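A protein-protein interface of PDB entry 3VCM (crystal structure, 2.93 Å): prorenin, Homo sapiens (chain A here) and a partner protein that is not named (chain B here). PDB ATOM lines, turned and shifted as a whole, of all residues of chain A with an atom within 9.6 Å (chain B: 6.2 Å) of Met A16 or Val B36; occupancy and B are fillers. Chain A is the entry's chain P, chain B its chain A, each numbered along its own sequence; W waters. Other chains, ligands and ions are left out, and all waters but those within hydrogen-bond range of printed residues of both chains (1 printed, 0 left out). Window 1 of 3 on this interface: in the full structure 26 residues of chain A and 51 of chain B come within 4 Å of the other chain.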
ATOM      1  N   ILE A  11      26.796  -1.113  12.442  1.00  0.00           N
ATOM      2  CA  ILE A  11      26.299   0.109  13.086  1.00  0.00           C
ATOM      3  C   ILE A  11      24.896  -0.253  13.562  1.00  0.00           C
ATOM      4  O   ILE A  11      24.009  -0.455  12.731  1.00  0.00           O
ATOM      5  CB  ILE A  11      26.278   1.360  12.152  1.00  0.00           C
ATOM      6  CG1 ILE A  11      27.692   1.745  11.664  1.00  0.00           C
ATOM      7  CG2 ILE A  11      25.597   2.551  12.859  1.00  0.00           C
ATOM      8  CD1 ILE A  11      27.729   2.735  10.462  1.00  0.00           C
ATOM      9  N   LEU A  13      21.316   0.289  14.616  1.00  0.00           N
ATOM     10  CA  LEU A  13      20.268   1.298  14.516  1.00  0.00           C
ATOM     11  C   LEU A  13      19.242   1.092  15.626  1.00  0.00           C
ATOM     12  O   LEU A  13      18.599   0.042  15.700  1.00  0.00           O
ATOM     13  CB  LEU A  13      19.614   1.340  13.120  1.00  0.00           C
ATOM     14  CG  LEU A  13      20.521   1.776  11.956  1.00  0.00           C
ATOM     15  CD1 LEU A  13      19.739   1.823  10.666  1.00  0.00           C
ATOM     16  CD2 LEU A  13      21.158   3.141  12.208  1.00  0.00           C
ATOM     17  N   LYS A  14      19.147   2.079  16.522  1.00  0.00           N
ATOM     18  CA  LYS A  14      18.282   2.061  17.697  1.00  0.00           C
ATOM     19  C   LYS A  14      17.006   2.859  17.434  1.00  0.00           C
ATOM     20  O   LYS A  14      17.059   3.905  16.784  1.00  0.00           O
ATOM     21  CB  LYS A  14      19.046   2.595  18.929  1.00  0.00           C
ATOM     22  CG  LYS A  14      20.512   2.140  18.976  1.00  0.00           C
ATOM     23  CD  LYS A  14      21.224   2.500  20.273  1.00  0.00           C
ATOM     24  CE  LYS A  14      22.661   2.015  20.283  1.00  0.00           C
ATOM     25  NZ  LYS A  14      23.560   2.877  19.465  1.00  0.00           N
ATOM     26  N   ARG A  15      15.861   2.352  17.930  1.00  0.00           N
ATOM     27  CA  ARG A  15      14.553   2.986  17.747  1.00  0.00           C
ATOM     28  C   ARG A  15      14.396   4.276  18.546  1.00  0.00           C
ATOM     29  O   ARG A  15      14.680   4.309  19.747  1.00  0.00           O
ATOM     30  CB  ARG A  15      13.409   2.017  18.069  1.00  0.00           C
ATOM     31  CG  ARG A  15      12.233   2.044  17.087  1.00  0.00           C
ATOM     32  CD  ARG A  15      11.295   3.212  17.317  1.00  0.00           C
ATOM     33  NE  ARG A  15      10.039   3.078  16.580  1.00  0.00           N
ATOM     34  CZ  ARG A  15       9.194   4.083  16.370  1.00  0.00           C
ATOM     35  NH1 ARG A  15       9.474   5.303  16.810  1.00  0.00           N
ATOM     36  NH2 ARG A  15       8.067   3.877  15.700  1.00  0.00           N
ATOM     37  N   MET A  16      13.921   5.330  17.866  1.00  0.00           N
ATOM     38  CA  MET A  16      13.668   6.655  18.431  1.00  0.00           C
ATOM     39  C   MET A  16      12.298   7.173  17.962  1.00  0.00           C
ATOM     40  O   MET A  16      11.846   6.762  16.889  1.00  0.00           O
ATOM     41  CB  MET A  16      14.785   7.648  18.030  1.00  0.00           C
ATOM     42  CG  MET A  16      14.934   7.885  16.525  1.00  0.00           C
ATOM     43  SD  MET A  16      15.849   9.397  16.130  1.00  0.00           S
ATOM     44  CE  MET A  16      15.848   9.312  14.372  1.00  0.00           C
ATOM     45  N   PRO A  17      11.624   8.083  18.704  1.00  0.00           N
ATOM     46  CA  PRO A  17      10.359   8.623  18.187  1.00  0.00           C
ATOM     47  C   PRO A  17      10.615   9.652  17.088  1.00  0.00           C
ATOM     48  O   PRO A  17      11.418  10.568  17.278  1.00  0.00           O
ATOM     49  CB  PRO A  17       9.692   9.238  19.419  1.00  0.00           C
ATOM     50  CG  PRO A  17      10.796   9.541  20.354  1.00  0.00           C
ATOM     51  CD  PRO A  17      11.989   8.694  20.000  1.00  0.00           C
ATOM     52  N   SER A  18       9.953   9.489  15.932  1.00  0.00           N
ATOM     53  CA  SER A  18      10.094  10.415  14.807  1.00  0.00           C
ATOM     54  C   SER A  18       9.476  11.781  15.147  1.00  0.00           C
ATOM     55  O   SER A  18       8.689  11.882  16.095  1.00  0.00           O
ATOM     56  CB  SER A  18       9.456   9.837  13.545  1.00  0.00           C
ATOM     57  OG  SER A  18       8.050  10.020  13.504  1.00  0.00           O
ATOM     58  N   ILE A  19       9.836  12.825  14.375  1.00  0.00           N
ATOM     59  CA  ILE A  19       9.329  14.183  14.571  1.00  0.00           C
ATOM     60  C   ILE A  19       7.797  14.181  14.500  1.00  0.00           C
ATOM     61  O   ILE A  19       7.153  14.721  15.402  1.00  0.00           O
ATOM     62  CB  ILE A  19      10.017  15.212  13.629  1.00  0.00           C
ATOM     63  CG1 ILE A  19      11.534  15.303  13.940  1.00  0.00           C
ATOM     64  CG2 ILE A  19       9.350  16.592  13.739  1.00  0.00           C
ATOM     65  CD1 ILE A  19      12.407  16.081  12.936  1.00  0.00           C
ATOM     66  N   ARG A  20       7.232  13.490  13.482  1.00  0.00           N
ATOM     67  CA  ARG A  20       5.787  13.332  13.256  1.00  0.00           C
ATOM     68  C   ARG A  20       5.119  12.703  14.488  1.00  0.00           C
ATOM     69  O   ARG A  20       4.128  13.246  14.983  1.00  0.00           O
ATOM     70  CB  ARG A  20       5.527  12.490  11.988  1.00  0.00           C
ATOM     71  CG  ARG A  20       4.055  12.240  11.681  1.00  0.00           C
ATOM     72  CD  ARG A  20       3.729  12.425  10.201  1.00  0.00           C
ATOM     73  NE  ARG A  20       2.392  12.968   9.911  1.00  0.00           N
ATOM     74  CZ  ARG A  20       1.720  13.870  10.635  1.00  0.00           C
ATOM     75  NH1 ARG A  20       2.240  14.340  11.769  1.00  0.00           N
ATOM     76  NH2 ARG A  20       0.531  14.297  10.246  1.00  0.00           N
ATOM     77  N   GLU A  21       5.688  11.586  14.991  1.00  0.00           N
ATOM     78  CA  GLU A  21       5.224  10.852  16.173  1.00  0.00           C
ATOM     79  C   GLU A  21       5.208  11.735  17.418  1.00  0.00           C
ATOM     80  O   GLU A  21       4.257  11.656  18.196  1.00  0.00           O
ATOM     81  CB  GLU A  21       6.105   9.619  16.434  1.00  0.00           C
ATOM     82  CG  GLU A  21       5.855   8.446  15.506  1.00  0.00           C
ATOM     83  CD  GLU A  21       6.787   7.271  15.719  1.00  0.00           C
ATOM     84  OE1 GLU A  21       8.021   7.466  15.618  1.00  0.00           O
ATOM     85  OE2 GLU A  21       6.283   6.150  15.960  1.00  0.00           O
ATOM     86  N   SER A  22       6.262  12.561  17.606  1.00  0.00           N
ATOM     87  CA  SER A  22       6.402  13.482  18.739  1.00  0.00           C
ATOM     88  C   SER A  22       5.335  14.577  18.691  1.00  0.00           C
ATOM     89  O   SER A  22       4.752  14.901  19.724  1.00  0.00           O
ATOM     90  CB  SER A  22       7.797  14.105  18.770  1.00  0.00           C
ATOM     91  OG  SER A  22       8.814  13.128  18.934  1.00  0.00           O
ATOM     92  N   TYR B  15      13.672  13.399   7.429  1.00  0.00           N
ATOM     93  CA  TYR B  15      13.688  13.268   8.894  1.00  0.00           C
ATOM     94  C   TYR B  15      12.367  13.514   9.651  1.00  0.00           C
ATOM     95  O   TYR B  15      12.334  13.323  10.869  1.00  0.00           O
ATOM     96  CB  TYR B  15      14.895  13.960   9.568  1.00  0.00           C
ATOM     97  CG  TYR B  15      16.120  14.171   8.698  1.00  0.00           C
ATOM     98  CD1 TYR B  15      16.734  13.100   8.048  1.00  0.00           C
ATOM     99  CD2 TYR B  15      16.707  15.425   8.582  1.00  0.00           C
ATOM    100  CE1 TYR B  15      17.862  13.292   7.251  1.00  0.00           C
ATOM    101  CE2 TYR B  15      17.842  15.625   7.806  1.00  0.00           C
ATOM    102  CZ  TYR B  15      18.413  14.557   7.137  1.00  0.00           C
ATOM    103  OH  TYR B  15      19.527  14.765   6.363  1.00  0.00           O
ATOM    104  N   THR B  18      11.415   9.332  10.735  1.00  0.00           N
ATOM    105  CA  THR B  18      12.701   8.649  10.886  1.00  0.00           C
ATOM    106  C   THR B  18      12.666   8.073  12.286  1.00  0.00           C
ATOM    107  O   THR B  18      12.689   8.822  13.266  1.00  0.00           O
ATOM    108  CB  THR B  18      13.912   9.584  10.644  1.00  0.00           C
ATOM    109  OG1 THR B  18      13.771  10.219   9.383  1.00  0.00           O
ATOM    110  CG2 THR B  18      15.243   8.832  10.644  1.00  0.00           C
ATOM    111  N   GLN B  19      12.556   6.748  12.377  1.00  0.00           N
ATOM    112  CA  GLN B  19      12.455   6.058  13.654  1.00  0.00           C
ATOM    113  C   GLN B  19      13.790   5.466  14.120  1.00  0.00           C
ATOM    114  O   GLN B  19      13.845   4.906  15.216  1.00  0.00           O
ATOM    115  CB  GLN B  19      11.380   4.959  13.576  1.00  0.00           C
ATOM    116  CG  GLN B  19      10.016   5.443  13.079  1.00  0.00           C
ATOM    117  CD  GLN B  19       9.277   4.351  12.356  1.00  0.00           C
ATOM    118  OE1 GLN B  19       8.311   3.789  12.871  1.00  0.00           O
ATOM    119  NE2 GLN B  19       9.714   4.028  11.138  1.00  0.00           N
ATOM    120  N   TYR B  20      14.864   5.590  13.308  1.00  0.00           N
ATOM    121  CA  TYR B  20      16.148   4.977  13.645  1.00  0.00           C
ATOM    122  C   TYR B  20      17.367   5.876  13.598  1.00  0.00           C
ATOM    123  O   TYR B  20      17.613   6.556  12.599  1.00  0.00           O
ATOM    124  CB  TYR B  20      16.379   3.697  12.824  1.00  0.00           C
ATOM    125  CG  TYR B  20      15.287   2.668  13.023  1.00  0.00           C
ATOM    126  CD1 TYR B  20      15.241   1.888  14.176  1.00  0.00           C
ATOM    127  CD2 TYR B  20      14.265   2.515  12.090  1.00  0.00           C
ATOM    128  CE1 TYR B  20      14.211   0.978  14.394  1.00  0.00           C
ATOM    129  CE2 TYR B  20      13.233   1.594  12.293  1.00  0.00           C
ATOM    130  CZ  TYR B  20      13.214   0.822  13.447  1.00  0.00           C
ATOM    131  OH  TYR B  20      12.213  -0.100  13.663  1.00  0.00           O
ATOM    132  N   TYR B  21      18.154   5.835  14.683  1.00  0.00           N
ATOM    133  CA  TYR B  21      19.401   6.585  14.818  1.00  0.00           C
ATOM    134  C   TYR B  21      20.586   5.642  15.058  1.00  0.00           C
ATOM    135  O   TYR B  21      20.405   4.510  15.513  1.00  0.00           O
ATOM    136  CB  TYR B  21      19.307   7.626  15.956  1.00  0.00           C
ATOM    137  CG  TYR B  21      19.405   7.039  17.350  1.00  0.00           C
ATOM    138  CD1 TYR B  21      18.262   6.729  18.080  1.00  0.00           C
ATOM    139  CD2 TYR B  21      20.640   6.807  17.946  1.00  0.00           C
ATOM    140  CE1 TYR B  21      18.347   6.200  19.367  1.00  0.00           C
ATOM    141  CE2 TYR B  21      20.739   6.237  19.212  1.00  0.00           C
ATOM    142  CZ  TYR B  21      19.589   5.954  19.928  1.00  0.00           C
ATOM    143  OH  TYR B  21      19.691   5.416  21.190  1.00  0.00           O
ATOM    144  N   GLY B  22      21.782   6.157  14.805  1.00  0.00           N
ATOM    145  CA  GLY B  22      23.041   5.481  15.063  1.00  0.00           C
ATOM    146  C   GLY B  22      23.916   6.376  15.913  1.00  0.00           C
ATOM    147  O   GLY B  22      23.585   7.544  16.120  1.00  0.00           O
ATOM    148  N   LYS B  34      23.761  11.161  18.612  1.00  0.00           N
ATOM    149  CA  LYS B  34      22.746  10.330  17.983  1.00  0.00           C
ATOM    150  C   LYS B  34      22.659  10.940  16.587  1.00  0.00           C
ATOM    151  O   LYS B  34      22.448  12.152  16.466  1.00  0.00           O
ATOM    152  CB  LYS B  34      21.393  10.448  18.706  1.00  0.00           C
ATOM    153  CG  LYS B  34      21.408  10.026  20.168  1.00  0.00           C
ATOM    154  CD  LYS B  34      20.101   9.343  20.530  1.00  0.00           C
ATOM    155  CE  LYS B  34      19.559   9.693  21.888  1.00  0.00           C
ATOM    156  NZ  LYS B  34      20.450   9.249  23.000  1.00  0.00           N
ATOM    157  N   VAL B  35      22.915  10.144  15.547  1.00  0.00           N
ATOM    158  CA  VAL B  35      22.912  10.637  14.168  1.00  0.00           C
ATOM    159  C   VAL B  35      22.035   9.813  13.245  1.00  0.00           C
ATOM    160  O   VAL B  35      21.911   8.604  13.423  1.00  0.00           O
ATOM    161  CB  VAL B  35      24.345  10.820  13.582  1.00  0.00           C
ATOM    162  CG1 VAL B  35      25.042  12.023  14.193  1.00  0.00           C
ATOM    163  CG2 VAL B  35      25.182   9.558  13.754  1.00  0.00           C
ATOM    164  N   VAL B  36      21.445  10.474  12.242  1.00  0.00           N
ATOM    165  CA  VAL B  36      20.626   9.831  11.220  1.00  0.00           C
ATOM    166  C   VAL B  36      21.564   9.466  10.066  1.00  0.00           C
ATOM    167  O   VAL B  36      22.304  10.323   9.573  1.00  0.00           O
ATOM    168  CB  VAL B  36      19.439  10.734  10.770  1.00  0.00           C
ATOM    169  CG1 VAL B  36      18.886  10.314   9.408  1.00  0.00           C
ATOM    170  CG2 VAL B  36      18.332  10.739  11.811  1.00  0.00           C
ATOM    171  N   PHE B  37      21.567   8.187   9.673  1.00  0.00           N
ATOM    172  CA  PHE B  37      22.397   7.709   8.578  1.00  0.00           C
ATOM    173  C   PHE B  37      21.576   7.793   7.308  1.00  0.00           C
ATOM    174  O   PHE B  37      20.682   6.974   7.075  1.00  0.00           O
ATOM    175  CB  PHE B  37      22.922   6.303   8.871  1.00  0.00           C
ATOM    176  CG  PHE B  37      24.039   6.310   9.885  1.00  0.00           C
ATOM    177  CD1 PHE B  37      23.764   6.306  11.246  1.00  0.00           C
ATOM    178  CD2 PHE B  37      25.367   6.329   9.479  1.00  0.00           C
ATOM    179  CE1 PHE B  37      24.796   6.329  12.179  1.00  0.00           C
ATOM    180  CE2 PHE B  37      26.398   6.338  10.415  1.00  0.00           C
ATOM    181  CZ  PHE B  37      26.106   6.352  11.759  1.00  0.00           C
ATOM    182  N   ASP B  38      21.835   8.853   6.534  1.00  0.00           N
ATOM    183  CA  ASP B  38      21.100   9.217   5.329  1.00  0.00           C
ATOM    184  C   ASP B  38      21.919   8.961   4.074  1.00  0.00           C
ATOM    185  O   ASP B  38      22.996   9.538   3.909  1.00  0.00           O
ATOM    186  CB  ASP B  38      20.688  10.707   5.432  1.00  0.00           C
ATOM    187  CG  ASP B  38      19.892  11.298   4.284  1.00  0.00           C
ATOM    188  OD1 ASP B  38      19.201  10.537   3.586  1.00  0.00           O
ATOM    189  OD2 ASP B  38      19.907  12.538   4.130  1.00  0.00           O
ATOM    190  N   ALA B 122      13.299  16.729  17.196  1.00  0.00           N
ATOM    191  CA  ALA B 122      14.189  15.699  16.672  1.00  0.00           C
ATOM    192  C   ALA B 122      14.905  15.061  17.851  1.00  0.00           C
ATOM    193  O   ALA B 122      15.524  15.776  18.640  1.00  0.00           O
ATOM    194  CB  ALA B 122      15.201  16.326  15.728  1.00  0.00           C
ATOM    195  N   GLU B 123      14.787  13.733  18.006  1.00  0.00           N
ATOM    196  CA  GLU B 123      15.437  13.008  19.100  1.00  0.00           C
ATOM    197  C   GLU B 123      16.933  12.783  18.816  1.00  0.00           C
ATOM    198  O   GLU B 123      17.705  12.524  19.742  1.00  0.00           O
ATOM    199  CB  GLU B 123      14.694  11.695  19.418  1.00  0.00           C
ATOM    200  CG  GLU B 123      14.342  11.544  20.894  1.00  0.00           C
ATOM    201  CD  GLU B 123      13.341  12.536  21.473  1.00  0.00           C
ATOM    202  OE1 GLU B 123      12.402  12.940  20.744  1.00  0.00           O
ATOM    203  OE2 GLU B 123      13.487  12.893  22.666  1.00  0.00           O
ATOM    204  N   PHE B 124      17.331  12.911  17.537  1.00  0.00           N
ATOM    205  CA  PHE B 124      18.710  12.803  17.054  1.00  0.00           C
ATOM    206  C   PHE B 124      19.381  14.172  17.100  1.00  0.00           C
ATOM    207  O   PHE B 124      18.700  15.196  17.028  1.00  0.00           O
ATOM    208  CB  PHE B 124      18.753  12.230  15.621  1.00  0.00           C
ATOM    209  CG  PHE B 124      18.048  13.054  14.565  1.00  0.00           C
ATOM    210  CD1 PHE B 124      16.678  12.925  14.354  1.00  0.00           C
ATOM    211  CD2 PHE B 124      18.761  13.927  13.750  1.00  0.00           C
ATOM    212  CE1 PHE B 124      16.030  13.680  13.373  1.00  0.00           C
ATOM    213  CE2 PHE B 124      18.110  14.681  12.768  1.00  0.00           C
ATOM    214  CZ  PHE B 124      16.750  14.557  12.592  1.00  0.00           C
ATOM    215  N   GLY B 126      22.466  15.066  15.080  1.00  0.00           N
ATOM    216  CA  GLY B 126      22.940  15.417  13.748  1.00  0.00           C
ATOM    217  C   GLY B 126      22.709  14.386  12.665  1.00  0.00           C
ATOM    218  O   GLY B 126      21.919  13.457  12.832  1.00  0.00           O
ATOM    219  N   VAL B 127      23.402  14.564  11.528  1.00  0.00           N
ATOM    220  CA  VAL B 127      23.269  13.731  10.331  1.00  0.00           C
ATOM    221  C   VAL B 127      24.637  13.243   9.836  1.00  0.00           C
ATOM    222  O   VAL B 127      25.606  14.001   9.842  1.00  0.00           O
ATOM    223  CB  VAL B 127      22.480  14.519   9.233  1.00  0.00           C
ATOM    224  CG1 VAL B 127      22.595  13.885   7.855  1.00  0.00           C
ATOM    225  CG2 VAL B 127      21.023  14.683   9.618  1.00  0.00           C
ATOM    226  N   VAL B 128      24.694  11.971   9.404  1.00  0.00           N
ATOM    227  CA  VAL B 128      25.868  11.342   8.797  1.00  0.00           C
ATOM    228  C   VAL B 128      25.466  10.902   7.377  1.00  0.00           C
ATOM    229  O   VAL B 128      24.675   9.970   7.201  1.00  0.00           O
ATOM    230  CB  VAL B 128      26.465  10.203   9.676  1.00  0.00           C
ATOM    231  CG1 VAL B 128      27.455   9.354   8.895  1.00  0.00           C
ATOM    232  CG2 VAL B 128      27.137  10.778  10.915  1.00  0.00           C
ATOM    233  N   GLY B 129      25.973  11.640   6.392  1.00  0.00           N
ATOM    234  CA  GLY B 129      25.686  11.435   4.979  1.00  0.00           C
ATOM    235  C   GLY B 129      26.429  10.272   4.367  1.00  0.00           C
ATOM    236  O   GLY B 129      27.664  10.275   4.315  1.00  0.00           O
ATOM    237  N   THR B 222      17.795   6.463   2.967  1.00  0.00           N
ATOM    238  CA  THR B 222      17.681   5.779   4.265  1.00  0.00           C
ATOM    239  C   THR B 222      17.208   6.704   5.380  1.00  0.00           C
ATOM    240  O   THR B 222      16.663   6.220   6.375  1.00  0.00           O
ATOM    241  CB  THR B 222      18.977   5.072   4.653  1.00  0.00           C
ATOM    242  OG1 THR B 222      20.033   6.029   4.715  1.00  0.00           O
ATOM    243  CG2 THR B 222      19.325   3.937   3.703  1.00  0.00           C
ATOM    244  N   GLY B 223      17.429   8.010   5.208  1.00  0.00           N
ATOM    245  CA  GLY B 223      16.995   9.044   6.143  1.00  0.00           C
ATOM    246  C   GLY B 223      15.485   9.173   6.131  1.00  0.00           C
ATOM    247  O   GLY B 223      14.876   9.513   7.149  1.00  0.00           O
ATOM    248  N   ALA B 224      14.876   8.877   4.969  1.00  0.00           N
ATOM    249  CA  ALA B 224      13.433   8.864   4.755  1.00  0.00           C
ATOM    250  C   ALA B 224      12.831   7.582   5.354  1.00  0.00           C
ATOM    251  O   ALA B 224      13.572   6.659   5.706  1.00  0.00           O
ATOM    252  CB  ALA B 224      13.135   8.935   3.263  1.00  0.00           C
HETATM  253  O   HOH W   1      13.656  12.125  16.204  1.00  0.00           O
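Of the 11 printed residues of chain A, 9 touch a printed residue of chain B.
Printed residues of chain B that touch a printed residue of chain A: Tyr B15, Thr B18, Gln B19, Tyr B20, Tyr B21, Val B36, Phe B37, Ala B122, Glu B123 and Phe B124.
Among the printed residues, no Asp or Glu carboxylate lies within 4 Å of a Lys or Arg side-chain nitrogen of the other chain.
Of the printed residues of chain B, Lys A14 touches Gln B19, Tyr B20 and Tyr B21.
Of chain B, only Thr B18 (3.4 Å), Gln B19 (2.7 Å), Tyr B20 (3.7 Å), Tyr B21 (3.6 Å), Val B36 (3.8 Å) and Phe B124 (3.7 Å) come within 4 Å of Met A16.
Of the printed residues of chain A, Gln B19 touches Lys A14, Arg A15, Met A16 and Glu A21.
No residue of chain A comes within 4 Å of Val B35.
Of chain A, only Met A16 comes within 4 Å of Val B36.
No residue of chain A comes within 4 Å of Val B127.
No residue of chain A comes within 4 Å of Val B128.
Thr B222 touches none of the printed residues of chain A.
The side-chain amide oxygen (OE1) of Gln B19 is in hydrogen-bond range of the guanidinium group (NH2) of Arg A15, at 2.8 Å.
The backbone carbonyl oxygen (O) of Gln B19 sits at hydrogen-bond distance from the backbone NH (N) of Met A16.
The backbone carbonyl oxygen (O) of Tyr B21 is in hydrogen-bond range of the backbone NH (N) of Lys A14 (2.9 Å).
Water W1 lies within hydrogen-bond range of the backbone NH (N) of Glu B123, the backbone carbonyl oxygen (O) of Pro A17 and the side-chain sulfur (SD) of Met A16.
Phe B37 touches Ile A11.
Lys A14 touches Gln B19.
Arg A15 touches Tyr B20.
CE of Met A16 touches O of Thr B18 (3.4 Å).
Tyr B20 touches Met A16 (O to CE, 3.7 Å).
Met A16 touches Tyr B21 (CB to CD1, 3.6 Å).
CG2 of Val B36 touches CE of Met A16, 3.8 Å away.
CB of Ser A18 touches O of Thr B18, 3.4 Å away.
Ile A19 touches Tyr B15 (CD1 to O, 3.4 Å).
CG1 of Ile A19 touches CA of Ala B122 (3.8 Å).
The side-chain carboxylate (OD2) of Asp B38 lies within hydrogen-bond range of the side-chain hydroxyl (OH) of Tyr B15 (3.2 Å).
The side-chain hydroxyl (OG1) of Thr B18 sits at hydrogen-bond distance from the backbone carbonyl oxygen (O) of Gly B223 (2.6 Å).
O of Gly B126 is in hydrogen-bond range of N of Val B36 (3.1 Å).
The backbone carbonyl oxygen of Val B36 is in hydrogen-bond range of the backbone NH of Val B128 (2.9 Å).
O of Phe B37 lies within hydrogen-bond range of OG1 of Thr B222, at 2.6 Å.
O of Ser A18 lies within hydrogen-bond range of OG of Ser A22.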
